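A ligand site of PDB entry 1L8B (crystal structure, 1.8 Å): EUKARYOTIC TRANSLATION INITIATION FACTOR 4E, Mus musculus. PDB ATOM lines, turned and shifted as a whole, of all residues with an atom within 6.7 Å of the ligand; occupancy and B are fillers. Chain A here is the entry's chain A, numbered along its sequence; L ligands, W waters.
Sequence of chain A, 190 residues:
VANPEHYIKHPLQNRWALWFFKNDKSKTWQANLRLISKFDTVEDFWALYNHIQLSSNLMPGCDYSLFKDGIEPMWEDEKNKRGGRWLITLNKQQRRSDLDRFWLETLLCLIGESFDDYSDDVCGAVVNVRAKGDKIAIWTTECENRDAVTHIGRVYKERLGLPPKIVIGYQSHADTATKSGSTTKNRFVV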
ATOM      1  N   PHE A  21      18.172 -30.975 -12.890  1.00  0.00           N
ATOM      2  CA  PHE A  21      18.250 -29.760 -13.689  1.00  0.00           C
ATOM      3  C   PHE A  21      19.217 -28.785 -13.046  1.00  0.00           C
ATOM      4  O   PHE A  21      19.183 -28.590 -11.827  1.00  0.00           O
ATOM      5  CB  PHE A  21      16.880 -29.088 -13.796  1.00  0.00           C
ATOM      6  CG  PHE A  21      16.901 -27.778 -14.543  1.00  0.00           C
ATOM      7  CD1 PHE A  21      16.746 -27.743 -15.930  1.00  0.00           C
ATOM      8  CD2 PHE A  21      17.108 -26.572 -13.870  1.00  0.00           C
ATOM      9  CE1 PHE A  21      16.787 -26.532 -16.626  1.00  0.00           C
ATOM     10  CE2 PHE A  21      17.155 -25.358 -14.553  1.00  0.00           C
ATOM     11  CZ  PHE A  21      16.998 -25.337 -15.936  1.00  0.00           C
ATOM     12  N   THR A  28      20.111 -23.749 -23.446  1.00  0.00           N
ATOM     13  CA  THR A  28      18.664 -23.649 -23.548  1.00  0.00           C
ATOM     14  C   THR A  28      18.115 -24.453 -22.373  1.00  0.00           C
ATOM     15  O   THR A  28      18.812 -25.338 -21.868  1.00  0.00           O
ATOM     16  CB  THR A  28      18.146 -24.255 -24.862  1.00  0.00           C
ATOM     17  OG1 THR A  28      16.740 -23.989 -24.986  1.00  0.00           O
ATOM     18  CG2 THR A  28      18.370 -25.750 -24.886  1.00  0.00           C
ATOM     19  N   TRP A  29      16.893 -24.152 -21.941  1.00  0.00           N
ATOM     20  CA  TRP A  29      16.320 -24.866 -20.797  1.00  0.00           C
ATOM     21  C   TRP A  29      16.369 -26.379 -20.976  1.00  0.00           C
ATOM     22  O   TRP A  29      16.831 -27.093 -20.080  1.00  0.00           O
ATOM     23  CB  TRP A  29      14.885 -24.415 -20.546  1.00  0.00           C
ATOM     24  CG  TRP A  29      14.293 -24.991 -19.281  1.00  0.00           C
ATOM     25  CD1 TRP A  29      14.374 -24.462 -18.025  1.00  0.00           C
ATOM     26  CD2 TRP A  29      13.582 -26.216 -19.159  1.00  0.00           C
ATOM     27  NE1 TRP A  29      13.747 -25.290 -17.117  1.00  0.00           N
ATOM     28  CE2 TRP A  29      13.250 -26.378 -17.789  1.00  0.00           C
ATOM     29  CE3 TRP A  29      13.185 -27.212 -20.075  1.00  0.00           C
ATOM     30  CZ2 TRP A  29      12.539 -27.494 -17.312  1.00  0.00           C
ATOM     31  CZ3 TRP A  29      12.480 -28.306 -19.597  1.00  0.00           C
ATOM     32  CH2 TRP A  29      12.166 -28.440 -18.225  1.00  0.00           C
ATOM     33  N   GLN A  30      15.893 -26.870 -22.112  1.00  0.00           N
ATOM     34  CA  GLN A  30      15.889 -28.312 -22.354  1.00  0.00           C
ATOM     35  C   GLN A  30      17.265 -28.975 -22.267  1.00  0.00           C
ATOM     36  O   GLN A  30      17.384 -30.105 -21.801  1.00  0.00           O
ATOM     37  CB  GLN A  30      15.275 -28.619 -23.726  1.00  0.00           C
ATOM     38  CG  GLN A  30      13.772 -28.545 -23.759  1.00  0.00           C
ATOM     39  CD  GLN A  30      13.199 -29.069 -25.066  1.00  0.00           C
ATOM     40  OE1 GLN A  30      13.590 -30.129 -25.538  1.00  0.00           O
ATOM     41  NE2 GLN A  30      12.273 -28.317 -25.654  1.00  0.00           N
ATOM     42  N   ASP A  63      16.934 -28.437  -9.813  1.00  0.00           N
ATOM     43  CA  ASP A  63      15.686 -29.154  -9.566  1.00  0.00           C
ATOM     44  C   ASP A  63      15.921 -30.664  -9.640  1.00  0.00           C
ATOM     45  O   ASP A  63      16.885 -31.124 -10.240  1.00  0.00           O
ATOM     46  CB  ASP A  63      14.600 -28.872 -10.615  1.00  0.00           C
ATOM     47  CG  ASP A  63      14.539 -27.416 -11.073  1.00  0.00           C
ATOM     48  OD1 ASP A  63      14.588 -26.500 -10.238  1.00  0.00           O
ATOM     49  OD2 ASP A  63      14.419 -27.211 -12.306  1.00  0.00           O
ATOM     50  N   PRO A  73      10.162 -34.618 -18.057  1.00  0.00           N
ATOM     51  CA  PRO A  73       9.665 -33.587 -17.138  1.00  0.00           C
ATOM     52  C   PRO A  73       9.600 -32.184 -17.716  1.00  0.00           C
ATOM     53  O   PRO A  73      10.196 -31.255 -17.174  1.00  0.00           O
ATOM     54  CB  PRO A  73      10.623 -33.700 -15.957  1.00  0.00           C
ATOM     55  CG  PRO A  73      11.921 -34.023 -16.631  1.00  0.00           C
ATOM     56  CD  PRO A  73      11.510 -35.070 -17.664  1.00  0.00           C
ATOM     57  N   MET A  74       8.869 -32.036 -18.816  1.00  0.00           N
ATOM     58  CA  MET A  74       8.735 -30.741 -19.475  1.00  0.00           C
ATOM     59  C   MET A  74       7.348 -30.523 -20.078  1.00  0.00           C
ATOM     60  O   MET A  74       6.650 -31.487 -20.410  1.00  0.00           O
ATOM     61  CB  MET A  74       9.796 -30.608 -20.572  1.00  0.00           C
ATOM     62  CG  MET A  74       9.872 -31.790 -21.518  1.00  0.00           C
ATOM     63  SD  MET A  74      11.237 -31.592 -22.693  1.00  0.00           S
ATOM     64  CE  MET A  74      10.397 -30.883 -24.066  1.00  0.00           C
ATOM     65  N   TRP A  75       6.955 -29.260 -20.206  1.00  0.00           N
ATOM     66  CA  TRP A  75       5.641 -28.906 -20.759  1.00  0.00           C
ATOM     67  C   TRP A  75       5.380 -29.482 -22.138  1.00  0.00           C
ATOM     68  O   TRP A  75       4.249 -29.820 -22.487  1.00  0.00           O
ATOM     69  CB  TRP A  75       5.486 -27.385 -20.881  1.00  0.00           C
ATOM     70  CG  TRP A  75       5.656 -26.592 -19.641  1.00  0.00           C
ATOM     71  CD1 TRP A  75       5.282 -26.951 -18.369  1.00  0.00           C
ATOM     72  CD2 TRP A  75       6.203 -25.271 -19.537  1.00  0.00           C
ATOM     73  NE1 TRP A  75       5.571 -25.936 -17.488  1.00  0.00           N
ATOM     74  CE2 TRP A  75       6.136 -24.894 -18.176  1.00  0.00           C
ATOM     75  CE3 TRP A  75       6.752 -24.371 -20.464  1.00  0.00           C
ATOM     76  CZ2 TRP A  75       6.594 -23.653 -17.724  1.00  0.00           C
ATOM     77  CZ3 TRP A  75       7.206 -23.138 -20.016  1.00  0.00           C
ATOM     78  CH2 TRP A  75       7.120 -22.789 -18.657  1.00  0.00           C
ATOM     79  N   GLU A  76       6.434 -29.582 -22.948  1.00  0.00           N
ATOM     80  CA  GLU A  76       6.317 -30.083 -24.311  1.00  0.00           C
ATOM     81  C   GLU A  76       5.927 -31.547 -24.487  1.00  0.00           C
ATOM     82  O   GLU A  76       5.396 -31.917 -25.529  1.00  0.00           O
ATOM     83  CB  GLU A  76       7.597 -29.784 -25.091  1.00  0.00           C
ATOM     84  CG  GLU A  76       7.935 -28.300 -25.196  1.00  0.00           C
ATOM     85  CD  GLU A  76       8.878 -27.814 -24.101  1.00  0.00           C
ATOM     86  OE1 GLU A  76       8.629 -28.076 -22.905  1.00  0.00           O
ATOM     87  OE2 GLU A  76       9.874 -27.144 -24.455  1.00  0.00           O
ATOM     88  N   ARG A  85      -0.320 -28.410 -12.695  1.00  0.00           N
ATOM     89  CA  ARG A  85       0.321 -28.842 -11.457  1.00  0.00           C
ATOM     90  C   ARG A  85      -0.317 -28.337 -10.168  1.00  0.00           C
ATOM     91  O   ARG A  85      -0.868 -27.231 -10.130  1.00  0.00           O
ATOM     92  CB  ARG A  85       1.757 -28.349 -11.457  1.00  0.00           C
ATOM     93  CG  ARG A  85       1.839 -26.920 -10.924  1.00  0.00           C
ATOM     94  CD  ARG A  85       2.605 -25.944 -11.791  1.00  0.00           C
ATOM     95  NE  ARG A  85       4.017 -25.889 -11.452  1.00  0.00           N
ATOM     96  CZ  ARG A  85       4.714 -24.759 -11.304  1.00  0.00           C
ATOM     97  NH1 ARG A  85       4.134 -23.578 -11.466  1.00  0.00           N
ATOM     98  NH2 ARG A  85       5.998 -24.809 -11.005  1.00  0.00           N
ATOM     99  N   ASN A 128      11.819 -27.527  -6.865  1.00  0.00           N
ATOM    100  CA  ASN A 128      12.681 -26.448  -7.354  1.00  0.00           C
ATOM    101  C   ASN A 128      13.354 -25.769  -6.164  1.00  0.00           C
ATOM    102  O   ASN A 128      12.676 -25.372  -5.221  1.00  0.00           O
ATOM    103  CB  ASN A 128      11.884 -25.349  -8.072  1.00  0.00           C
ATOM    104  CG  ASN A 128      11.054 -25.846  -9.238  1.00  0.00           C
ATOM    105  OD1 ASN A 128       9.845 -25.666  -9.258  1.00  0.00           O
ATOM    106  ND2 ASN A 128      11.696 -26.477 -10.219  1.00  0.00           N
ATOM    107  N   ARG A 130      15.308 -22.515  -5.039  1.00  0.00           N
ATOM    108  CA  ARG A 130      15.609 -21.163  -5.494  1.00  0.00           C
ATOM    109  C   ARG A 130      15.958 -20.222  -4.333  1.00  0.00           C
ATOM    110  O   ARG A 130      15.533 -20.433  -3.194  1.00  0.00           O
ATOM    111  CB  ARG A 130      14.415 -20.594  -6.263  1.00  0.00           C
ATOM    112  CG  ARG A 130      13.983 -21.434  -7.472  1.00  0.00           C
ATOM    113  CD  ARG A 130      14.947 -21.302  -8.644  1.00  0.00           C
ATOM    114  NE  ARG A 130      14.464 -22.000  -9.844  1.00  0.00           N
ATOM    115  CZ  ARG A 130      14.628 -23.300 -10.079  1.00  0.00           C
ATOM    116  NH1 ARG A 130      15.263 -24.062  -9.194  1.00  0.00           N
ATOM    117  NH2 ARG A 130      14.142 -23.841 -11.184  1.00  0.00           N
ATOM    118  N   GLY A 133      12.785 -18.825  -2.663  1.00  0.00           N
ATOM    119  CA  GLY A 133      11.944 -19.766  -1.952  1.00  0.00           C
ATOM    120  C   GLY A 133      11.814 -21.051  -2.745  1.00  0.00           C
ATOM    121  O   GLY A 133      11.893 -21.040  -3.972  1.00  0.00           O
ATOM    122  N   LYS A 135       9.923 -24.722  -4.079  1.00  0.00           N
ATOM    123  CA  LYS A 135       8.607 -25.166  -4.529  1.00  0.00           C
ATOM    124  C   LYS A 135       8.594 -26.664  -4.818  1.00  0.00           C
ATOM    125  O   LYS A 135       9.582 -27.228  -5.296  1.00  0.00           O
ATOM    126  CB  LYS A 135       8.190 -24.437  -5.818  1.00  0.00           C
ATOM    127  CG  LYS A 135       7.902 -22.947  -5.647  1.00  0.00           C
ATOM    128  CD  LYS A 135       7.617 -22.271  -6.991  1.00  0.00           C
ATOM    129  CE  LYS A 135       8.874 -22.180  -7.844  1.00  0.00           C
ATOM    130  NZ  LYS A 135       8.662 -21.407  -9.116  1.00  0.00           N
ATOM    131  N   TRP A 139       2.589 -32.912 -10.971  1.00  0.00           N
ATOM    132  CA  TRP A 139       2.127 -32.676 -12.334  1.00  0.00           C
ATOM    133  C   TRP A 139       1.083 -33.720 -12.772  1.00  0.00           C
ATOM    134  O   TRP A 139       1.282 -34.914 -12.565  1.00  0.00           O
ATOM    135  CB  TRP A 139       3.317 -32.744 -13.290  1.00  0.00           C
ATOM    136  CG  TRP A 139       4.241 -31.547 -13.248  1.00  0.00           C
ATOM    137  CD1 TRP A 139       4.534 -30.759 -12.165  1.00  0.00           C
ATOM    138  CD2 TRP A 139       4.992 -31.005 -14.341  1.00  0.00           C
ATOM    139  NE1 TRP A 139       5.418 -29.766 -12.520  1.00  0.00           N
ATOM    140  CE2 TRP A 139       5.710 -29.891 -13.852  1.00  0.00           C
ATOM    141  CE3 TRP A 139       5.114 -31.350 -15.693  1.00  0.00           C
ATOM    142  CZ2 TRP A 139       6.561 -29.123 -14.657  1.00  0.00           C
ATOM    143  CZ3 TRP A 139       5.953 -30.588 -16.500  1.00  0.00           C
ATOM    144  CH2 TRP A 139       6.667 -29.489 -15.983  1.00  0.00           C
ATOM    145  N   THR A 176       0.955 -21.013 -17.014  1.00  0.00           N
ATOM    146  CA  THR A 176       2.269 -20.768 -16.452  1.00  0.00           C
ATOM    147  C   THR A 176       3.247 -20.343 -17.542  1.00  0.00           C
ATOM    148  O   THR A 176       4.077 -19.457 -17.330  1.00  0.00           O
ATOM    149  CB  THR A 176       2.833 -22.034 -15.753  1.00  0.00           C
ATOM    150  OG1 THR A 176       1.919 -22.467 -14.746  1.00  0.00           O
ATOM    151  CG2 THR A 176       4.188 -21.737 -15.117  1.00  0.00           C
ATOM    152  N   ALA A 177       3.126 -20.948 -18.716  1.00  0.00           N
ATOM    153  CA  ALA A 177       3.994 -20.651 -19.841  1.00  0.00           C
ATOM    154  C   ALA A 177       3.803 -19.236 -20.381  1.00  0.00           C
ATOM    155  O   ALA A 177       4.735 -18.622 -20.891  1.00  0.00           O
ATOM    156  CB  ALA A 177       3.774 -21.659 -20.943  1.00  0.00           C
ATOM    157  N   LYS A 179       3.061 -16.274 -18.747  1.00  0.00           N
ATOM    158  CA  LYS A 179       2.973 -15.346 -17.625  1.00  0.00           C
ATOM    159  C   LYS A 179       2.830 -13.909 -18.113  1.00  0.00           C
ATOM    160  O   LYS A 179       3.316 -13.555 -19.182  1.00  0.00           O
ATOM    161  CB  LYS A 179       4.237 -15.462 -16.753  1.00  0.00           C
ATOM    162  CG  LYS A 179       4.479 -16.865 -16.229  1.00  0.00           C
ATOM    163  CD  LYS A 179       5.741 -16.937 -15.389  1.00  0.00           C
ATOM    164  CE  LYS A 179       5.923 -18.350 -14.845  1.00  0.00           C
ATOM    165  NZ  LYS A 179       7.095 -18.439 -13.944  1.00  0.00           N
HETATM  166  P1  LIG L   1      10.931 -22.431 -13.155  1.00  0.00           P
HETATM  167  O1  LIG L   1      12.286 -23.072 -13.245  1.00  0.00           O
HETATM  168  O2  LIG L   1       9.935 -23.528 -13.272  1.00  0.00           O
HETATM  169  O3  LIG L   1      10.745 -21.695 -11.721  1.00  0.00           O
HETATM  170  O4  LIG L   1      10.694 -21.389 -14.424  1.00  0.00           O
HETATM  171  P2  LIG L   1      11.392 -20.290 -11.277  1.00  0.00           P
HETATM  172  O5  LIG L   1      12.870 -20.312 -11.338  1.00  0.00           O
HETATM  173  O6  LIG L   1      10.966 -20.055  -9.877  1.00  0.00           O
HETATM  174  O7  LIG L   1      10.882 -19.197 -12.129  1.00  0.00           O
HETATM  175  P3  LIG L   1       9.725 -18.100 -12.308  1.00  0.00           P
HETATM  176  O8  LIG L   1       9.692 -17.810 -13.787  1.00  0.00           O
HETATM  177  O9  LIG L   1       9.975 -16.873 -11.509  1.00  0.00           O
HETATM  178  O10 LIG L   1       8.504 -18.824 -11.851  1.00  0.00           O
HETATM  179  C1  LIG L   1      11.744 -20.656 -15.043  1.00  0.00           C
HETATM  180  C2  LIG L   1      11.771 -20.675 -16.547  1.00  0.00           C
HETATM  181  O11 LIG L   1      12.218 -22.009 -16.996  1.00  0.00           O
HETATM  182  C3  LIG L   1      10.447 -20.575 -17.256  1.00  0.00           C
HETATM  183  O12 LIG L   1      10.001 -19.190 -17.338  1.00  0.00           O
HETATM  184  C4  LIG L   1      10.826 -21.074 -18.675  1.00  0.00           C
HETATM  185  O13 LIG L   1      11.580 -20.129 -19.498  1.00  0.00           O
HETATM  186  C5  LIG L   1      11.663 -22.301 -18.311  1.00  0.00           C
HETATM  187  N1  LIG L   1      10.897 -23.590 -18.010  1.00  0.00           N
HETATM  188  C6  LIG L   1      10.428 -24.153 -16.888  1.00  0.00           C
HETATM  189  N2  LIG L   1       9.840 -25.276 -17.182  1.00  0.00           N
HETATM  190  C7  LIG L   1       9.203 -26.173 -16.231  1.00  0.00           C
HETATM  191  C8  LIG L   1       9.870 -25.556 -18.640  1.00  0.00           C
HETATM  192  C9  LIG L   1       9.456 -26.483 -19.445  1.00  0.00           C
HETATM  193  O14 LIG L   1       8.802 -27.541 -19.053  1.00  0.00           O
HETATM  194  N3  LIG L   1       9.792 -26.199 -20.795  1.00  0.00           N
HETATM  195  C10 LIG L   1      10.486 -25.071 -21.236  1.00  0.00           C
HETATM  196  N4  LIG L   1      10.736 -24.930 -22.526  1.00  0.00           N
HETATM  197  N5  LIG L   1      10.906 -24.129 -20.398  1.00  0.00           N
HETATM  198  C11 LIG L   1      10.581 -24.382 -19.066  1.00  0.00           C
HETATM  199  O   HOH W   1      11.536 -18.462  -7.792  1.00  0.00           O
HETATM  200  O   HOH W   2       6.719 -21.317 -11.942  1.00  0.00           O
HETATM  201  O   HOH W   3      14.713 -22.574 -14.387  1.00  0.00           O
HETATM  202  O   HOH W   4       8.481 -26.593 -12.744  1.00  0.00           O
HETATM  203  O   HOH W   5      14.400 -19.049 -13.225  1.00  0.00           O
HETATM  204  O   HOH W   6      12.980 -25.661 -14.078  1.00  0.00           O
HETATM  205  O   HOH W   7       7.627 -22.888 -14.144  1.00  0.00           O
HETATM  206  O   HOH W   8      10.787 -27.624 -13.483  1.00  0.00           O
HETATM  207  O   HOH W   9       8.468 -23.780 -10.820  1.00  0.00           O
HETATM  208  O   HOH W  10       7.796 -20.578 -15.275  1.00  0.00           O
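NZ of Lys 179 lies within salt-bridge range of O10 of the ligand, 2.6 Å away. NE of Arg 130 is in salt-bridge range of O5 of the ligand, 2.8 Å away. N of Trp 75 lies within hydrogen-bond range of O14 of the ligand (2.8 Å). The side-chain amino group (NZ) of Lys 135 lies within salt-bridge range of an oxygen (O6) of the ligand, at 2.8 Å. The side-chain carboxylate (OE1) of Glu 76 is in hydrogen-bond range of a nitrogen (N3) of the ligand.
Water W3 bridges O1 of the ligand (2.7 Å) and NH2 of Arg 130 (3.5 Å). Water W6 lies within hydrogen-bond range of the side-chain carboxylate (OD2) of Asp 63, an oxygen (O1) of the ligand and the indole nitrogen (NE1) of Trp 29. Water W9 lies within hydrogen-bond range of NH2 of Arg 85 (2.7 Å), OD1 of Asn 128 (2.8 Å), O2 of the ligand (2.9 Å) and NZ of Lys 135 (2.9 Å). Water W2 lies within hydrogen-bond range of O10 of the ligand (3.1 Å), NZ of Lys 135 (3.4 Å) and NH1 of Arg 85 (3.5 Å). Water W10 lies within hydrogen-bond range of NZ of Lys 179 (2.6 Å) and O4 of the ligand (3.1 Å).
NH1 of Arg 130 lies within salt-bridge range of OD1 of Asp 63 (2.7 Å). O of Lys 135 lies within hydrogen-bond range of N of Asn 128 (2.7 Å). The side-chain carboxylate of Glu 76 is in hydrogen-bond range of the side-chain amide nitrogen of Gln 30 (2.9 Å).
N1 of the ligand lies close to NE1 of Trp 29 (3.4 Å). Residues that only touch the ligand: Met 74. Hydrophobic or aromatic side chains within 4 Å of the ligand: Trp 29, Met 74 and Trp 75. Of the 18 residues printed, 7 come within 4 Å of the ligand. The nearest printed residue that does not touch the ligand is Trp 139 (4.2 Å).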
